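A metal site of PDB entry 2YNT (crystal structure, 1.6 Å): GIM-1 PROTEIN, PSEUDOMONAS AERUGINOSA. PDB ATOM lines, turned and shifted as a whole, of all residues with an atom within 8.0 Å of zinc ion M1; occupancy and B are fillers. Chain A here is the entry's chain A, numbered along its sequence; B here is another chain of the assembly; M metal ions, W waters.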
ATOM      1  N   THR A  76       9.412  24.299  -5.620  1.00  0.00           N
ATOM      2  CA  THR A  76       8.051  24.761  -5.351  1.00  0.00           C
ATOM      3  C   THR A  76       7.899  25.717  -4.163  1.00  0.00           C
ATOM      4  O   THR A  76       6.822  26.245  -3.945  1.00  0.00           O
ATOM      5  CB  THR A  76       7.051  23.587  -5.238  1.00  0.00           C
ATOM      6  OG1 THR A  76       7.417  22.701  -4.172  1.00  0.00           O
ATOM      7  CG2 THR A  76       7.020  22.819  -6.556  1.00  0.00           C
ATOM      8  N   HIS A  77       8.969  25.883  -3.378  1.00  0.00           N
ATOM      9  CA  HIS A  77       9.154  27.028  -2.484  1.00  0.00           C
ATOM     10  C   HIS A  77      10.605  27.074  -2.047  1.00  0.00           C
ATOM     11  O   HIS A  77      11.398  26.245  -2.472  1.00  0.00           O
ATOM     12  CB  HIS A  77       8.147  27.086  -1.318  1.00  0.00           C
ATOM     13  CG  HIS A  77       8.206  25.932  -0.361  1.00  0.00           C
ATOM     14  ND1 HIS A  77       7.659  24.701  -0.631  1.00  0.00           N
ATOM     15  CD2 HIS A  77       8.720  25.845   0.893  1.00  0.00           C
ATOM     16  CE1 HIS A  77       7.821  23.903   0.407  1.00  0.00           C
ATOM     17  NE2 HIS A  77       8.466  24.567   1.346  1.00  0.00           N
ATOM     18  N   SER A  78      10.971  28.047  -1.210  1.00  0.00           N
ATOM     19  CA  SER A  78      12.385  28.291  -0.961  1.00  0.00           C
ATOM     20  C   SER A  78      13.018  27.393   0.103  1.00  0.00           C
ATOM     21  O   SER A  78      14.252  27.351   0.216  1.00  0.00           O
ATOM     22  CB  SER A  78      12.607  29.756  -0.582  1.00  0.00           C
ATOM     23  OG  SER A  78      12.065  30.022   0.698  1.00  0.00           O
ATOM     24  N   HIS A  79      12.210  26.668   0.867  1.00  0.00           N
ATOM     25  CA  HIS A  79      12.758  25.809   1.917  1.00  0.00           C
ATOM     26  C   HIS A  79      13.798  24.809   1.403  1.00  0.00           C
ATOM     27  O   HIS A  79      13.744  24.368   0.242  1.00  0.00           O
ATOM     28  CB  HIS A  79      11.644  25.036   2.629  1.00  0.00           C
ATOM     29  CG  HIS A  79      10.873  25.858   3.612  1.00  0.00           C
ATOM     30  ND1 HIS A  79       9.641  25.459   4.097  1.00  0.00           N
ATOM     31  CD2 HIS A  79      11.149  27.034   4.226  1.00  0.00           C
ATOM     32  CE1 HIS A  79       9.204  26.363   4.970  1.00  0.00           C
ATOM     33  NE2 HIS A  79      10.104  27.321   5.063  1.00  0.00           N
ATOM     34  N   GLU A  80      14.719  24.445   2.297  1.00  0.00           N
ATOM     35  CA  GLU A  80      15.809  23.526   1.994  1.00  0.00           C
ATOM     36  C   GLU A  80      15.344  22.204   1.366  1.00  0.00           C
ATOM     37  O   GLU A  80      15.986  21.688   0.459  1.00  0.00           O
ATOM     38  CB  GLU A  80      16.632  23.261   3.271  1.00  0.00           C
ATOM     39  CG  GLU A  80      17.878  22.389   3.074  1.00  0.00           C
ATOM     40  CD  GLU A  80      19.017  23.104   2.370  1.00  0.00           C
ATOM     41  OE1 GLU A  80      18.870  24.316   2.066  1.00  0.00           O
ATOM     42  OE2 GLU A  80      20.071  22.462   2.123  1.00  0.00           O
ATOM     43  N   ASP A  81      14.229  21.652   1.858  1.00  0.00           N
ATOM     44  CA  ASP A  81      13.781  20.374   1.336  1.00  0.00           C
ATOM     45  C   ASP A  81      13.301  20.436  -0.119  1.00  0.00           C
ATOM     46  O   ASP A  81      13.130  19.390  -0.743  1.00  0.00           O
ATOM     47  CB  ASP A  81      12.726  19.693   2.250  1.00  0.00           C
ATOM     48  CG  ASP A  81      11.523  20.578   2.542  1.00  0.00           C
ATOM     49  OD1 ASP A  81      11.669  21.594   3.244  1.00  0.00           O
ATOM     50  OD2 ASP A  81      10.388  20.196   2.129  1.00  0.00           O
ATOM     51  N   ARG A  82      13.108  21.639  -0.641  1.00  0.00           N
ATOM     52  CA  ARG A  82      12.743  21.837  -2.041  1.00  0.00           C
ATOM     53  C   ARG A  82      13.932  22.236  -2.926  1.00  0.00           C
ATOM     54  O   ARG A  82      13.874  22.072  -4.144  1.00  0.00           O
ATOM     55  CB  ARG A  82      11.703  22.951  -2.198  1.00  0.00           C
ATOM     56  CG  ARG A  82      10.484  22.851  -1.309  1.00  0.00           C
ATOM     57  CD  ARG A  82       9.614  21.661  -1.679  1.00  0.00           C
ATOM     58  NE  ARG A  82       9.829  20.512  -0.798  1.00  0.00           N
ATOM     59  CZ  ARG A  82       9.419  19.277  -1.079  1.00  0.00           C
ATOM     60  NH1 ARG A  82       8.861  19.007  -2.246  1.00  0.00           N
ATOM     61  NH2 ARG A  82       9.623  18.293  -0.203  1.00  0.00           N
ATOM     62  N   HIS A 139       1.410  27.024   3.396  1.00  0.00           N
ATOM     63  CA  HIS A 139       2.577  26.481   4.057  1.00  0.00           C
ATOM     64  C   HIS A 139       3.689  27.529   4.109  1.00  0.00           C
ATOM     65  O   HIS A 139       4.358  27.699   5.143  1.00  0.00           O
ATOM     66  CB  HIS A 139       3.055  25.217   3.324  1.00  0.00           C
ATOM     67  CG  HIS A 139       4.429  24.770   3.723  1.00  0.00           C
ATOM     68  ND1 HIS A 139       4.670  24.120   4.912  1.00  0.00           N
ATOM     69  CD2 HIS A 139       5.628  24.891   3.104  1.00  0.00           C
ATOM     70  CE1 HIS A 139       5.970  23.857   5.019  1.00  0.00           C
ATOM     71  NE2 HIS A 139       6.564  24.307   3.926  1.00  0.00           N
ATOM     72  N   THR A 140       3.879  28.221   2.990  1.00  0.00           N
ATOM     73  CA  THR A 140       4.754  29.394   2.934  1.00  0.00           C
ATOM     74  C   THR A 140       4.085  30.434   2.060  1.00  0.00           C
ATOM     75  O   THR A 140       3.058  30.175   1.424  1.00  0.00           O
ATOM     76  CB  THR A 140       6.131  29.085   2.331  1.00  0.00           C
ATOM     77  OG1 THR A 140       5.950  28.455   1.050  1.00  0.00           O
ATOM     78  CG2 THR A 140       6.944  28.178   3.254  1.00  0.00           C
ATOM     79  N   ASP A 142       5.214  31.571  -0.640  1.00  0.00           N
ATOM     80  CA  ASP A 142       5.587  31.416  -2.043  1.00  0.00           C
ATOM     81  C   ASP A 142       5.194  30.068  -2.644  1.00  0.00           C
ATOM     82  O   ASP A 142       5.447  29.830  -3.833  1.00  0.00           O
ATOM     83  CB  ASP A 142       7.098  31.645  -2.226  1.00  0.00           C
ATOM     84  CG  ASP A 142       7.957  30.701  -1.384  1.00  0.00           C
ATOM     85  OD1 ASP A 142       7.573  30.365  -0.244  1.00  0.00           O
ATOM     86  OD2 ASP A 142       9.038  30.294  -1.850  1.00  0.00           O
ATOM     87  N   ASN A 143       4.583  29.191  -1.850  1.00  0.00           N
ATOM     88  CA  ASN A 143       4.322  27.830  -2.342  1.00  0.00           C
ATOM     89  C   ASN A 143       3.533  27.755  -3.657  1.00  0.00           C
ATOM     90  O   ASN A 143       2.487  28.404  -3.817  1.00  0.00           O
ATOM     91  CB  ASN A 143       3.742  26.887  -1.256  1.00  0.00           C
ATOM     92  CG  ASN A 143       2.532  27.458  -0.505  1.00  0.00           C
ATOM     93  OD1 ASN A 143       2.321  27.133   0.665  1.00  0.00           O
ATOM     94  ND2 ASN A 143       1.706  28.276  -1.182  1.00  0.00           N
ATOM     95  N   GLY A 157       3.038  19.541  -3.222  1.00  0.00           N
ATOM     96  CA  GLY A 157       4.163  20.010  -2.430  1.00  0.00           C
ATOM     97  C   GLY A 157       3.760  20.142  -0.977  1.00  0.00           C
ATOM     98  O   GLY A 157       2.842  19.464  -0.498  1.00  0.00           O
ATOM     99  N   CYS A 158       4.439  21.024  -0.274  1.00  0.00           N
ATOM    100  CA  CYS A 158       4.280  21.084   1.180  1.00  0.00           C
ATOM    101  C   CYS A 158       3.051  21.890   1.574  1.00  0.00           C
ATOM    102  O   CYS A 158       2.686  21.936   2.737  1.00  0.00           O
ATOM    103  CB  CYS A 158       5.552  21.597   1.819  1.00  0.00           C
ATOM    104  SG  CYS A 158       6.983  20.642   1.217  1.00  0.00           S
ATOM    105  N   LEU A 159       2.389  22.484   0.567  1.00  0.00           N
ATOM    106  CA  LEU A 159       1.108  23.176   0.782  1.00  0.00           C
ATOM    107  C   LEU A 159       0.001  22.184   1.127  1.00  0.00           C
ATOM    108  O   LEU A 159      -0.970  22.535   1.797  1.00  0.00           O
ATOM    109  CB  LEU A 159       0.741  23.958  -0.485  1.00  0.00           C
ATOM    110  CG  LEU A 159      -0.642  24.622  -0.541  1.00  0.00           C
ATOM    111  CD1 LEU A 159      -0.761  25.631   0.604  1.00  0.00           C
ATOM    112  CD2 LEU A 159      -0.815  25.311  -1.869  1.00  0.00           C
ATOM    113  N   TYR A 170       5.369  22.013   9.942  1.00  0.00           N
ATOM    114  CA  TYR A 170       6.099  23.225  10.269  1.00  0.00           C
ATOM    115  C   TYR A 170       5.375  24.467   9.750  1.00  0.00           C
ATOM    116  O   TYR A 170       5.155  24.605   8.539  1.00  0.00           O
ATOM    117  CB  TYR A 170       7.520  23.159   9.707  1.00  0.00           C
ATOM    118  CG  TYR A 170       8.306  24.428   9.956  1.00  0.00           C
ATOM    119  CD1 TYR A 170       8.830  24.694  11.211  1.00  0.00           C
ATOM    120  CD2 TYR A 170       8.535  25.357   8.936  1.00  0.00           C
ATOM    121  CE1 TYR A 170       9.553  25.849  11.465  1.00  0.00           C
ATOM    122  CE2 TYR A 170       9.258  26.517   9.178  1.00  0.00           C
ATOM    123  CZ  TYR A 170       9.768  26.753  10.457  1.00  0.00           C
ATOM    124  OH  TYR A 170      10.491  27.888  10.741  1.00  0.00           O
ATOM    125  N   ASP A 173       6.888  29.532   8.824  1.00  0.00           N
ATOM    126  CA  ASP A 173       6.848  30.463   7.701  1.00  0.00           C
ATOM    127  C   ASP A 173       5.449  30.551   7.065  1.00  0.00           C
ATOM    128  O   ASP A 173       5.287  31.091   5.967  1.00  0.00           O
ATOM    129  CB  ASP A 173       7.898  30.071   6.656  1.00  0.00           C
ATOM    130  CG  ASP A 173       9.331  30.233   7.157  1.00  0.00           C
ATOM    131  OD1 ASP A 173       9.608  31.220   7.875  1.00  0.00           O
ATOM    132  OD2 ASP A 173      10.189  29.384   6.862  1.00  0.00           O
ATOM    133  N   HIS A 200       5.597  15.878   1.978  1.00  0.00           N
ATOM    134  CA  HIS A 200       6.010  14.988   3.063  1.00  0.00           C
ATOM    135  C   HIS A 200       4.886  13.990   3.303  1.00  0.00           C
ATOM    136  O   HIS A 200       3.736  14.384   3.454  1.00  0.00           O
ATOM    137  CB  HIS A 200       6.266  15.788   4.340  1.00  0.00           C
ATOM    138  CG  HIS A 200       7.265  16.883   4.176  1.00  0.00           C
ATOM    139  ND1 HIS A 200       8.617  16.663   4.207  1.00  0.00           N
ATOM    140  CD2 HIS A 200       7.115  18.216   3.957  1.00  0.00           C
ATOM    141  CE1 HIS A 200       9.265  17.800   4.012  1.00  0.00           C
ATOM    142  NE2 HIS A 200       8.377  18.757   3.847  1.00  0.00           N
ATOM    143  N   GLU B  26      11.933  23.023  10.554  1.00  0.00           N
ATOM    144  CA  GLU B  26      11.533  22.824   9.162  1.00  0.00           C
ATOM    145  C   GLU B  26      11.486  21.364   8.756  1.00  0.00           C
ATOM    146  O   GLU B  26      12.372  20.581   9.098  1.00  0.00           O
ATOM    147  CB  GLU B  26      12.508  23.540   8.225  1.00  0.00           C
ATOM    148  CG  GLU B  26      12.259  25.016   8.096  1.00  0.00           C
ATOM    149  CD  GLU B  26      13.104  25.637   7.011  1.00  0.00           C
ATOM    150  OE1 GLU B  26      13.379  24.952   6.000  1.00  0.00           O
ATOM    151  OE2 GLU B  26      13.487  26.816   7.172  1.00  0.00           O
ATOM    152  N   GLY B  27      10.460  21.001   7.982  1.00  0.00           N
ATOM    153  CA  GLY B  27      10.297  19.638   7.537  1.00  0.00           C
ATOM    154  C   GLY B  27       9.448  18.802   8.465  1.00  0.00           C
ATOM    155  O   GLY B  27       8.997  17.717   8.091  1.00  0.00           O
ATOM    156  N   TYR B  28       9.216  19.304   9.686  1.00  0.00           N
ATOM    157  CA  TYR B  28       8.435  18.548  10.657  1.00  0.00           C
ATOM    158  C   TYR B  28       7.467  19.371  11.519  1.00  0.00           C
ATOM    159  O   TYR B  28       6.284  19.060  11.575  1.00  0.00           O
ATOM    160  CB  TYR B  28       9.348  17.697  11.553  1.00  0.00           C
ATOM    161  CG  TYR B  28       8.560  16.985  12.627  1.00  0.00           C
ATOM    162  CD1 TYR B  28       7.834  15.842  12.331  1.00  0.00           C
ATOM    163  CD2 TYR B  28       8.523  17.468  13.937  1.00  0.00           C
ATOM    164  CE1 TYR B  28       7.097  15.191  13.298  1.00  0.00           C
ATOM    165  CE2 TYR B  28       7.789  16.825  14.915  1.00  0.00           C
ATOM    166  CZ  TYR B  28       7.075  15.689  14.577  1.00  0.00           C
ATOM    167  OH  TYR B  28       6.343  15.036  15.535  1.00  0.00           O
HETATM  168 ZN    ZN M   1       8.491  24.036   3.333  1.00  0.00          ZN
HETATM  169 ZN    ZN M   2       8.547  20.575   2.864  1.00  0.00          ZN
HETATM  170  O   HOH W   1       9.068  22.263   3.891  1.00  0.00           O
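Water W1 binds zinc ion M1 (1.9 Å). Zinc ion M1 is bound by ND1 of His 79 (2.0 Å). A ring nitrogen (NE2) of His 139 is bound to zinc ion M1 (2.0 Å). A ring nitrogen (NE2) of His 77 is bound to zinc ion M1. Zinc ion M1 has four donor atoms within binding distance.
Three residues have an atom within 4 Å of zinc ion M1: His 77, His 79 and His 139. The nearest printed residue that does not touch zinc ion M1 is Asp 81 (4.01 Å).
NE2 of His 79 lies within hydrogen-bond range of OD2 of Asp 173 (2.7 Å). The side-chain amide oxygen of Asn 143 sits at hydrogen-bond distance from the backbone NH of His 139 (2.9 Å).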
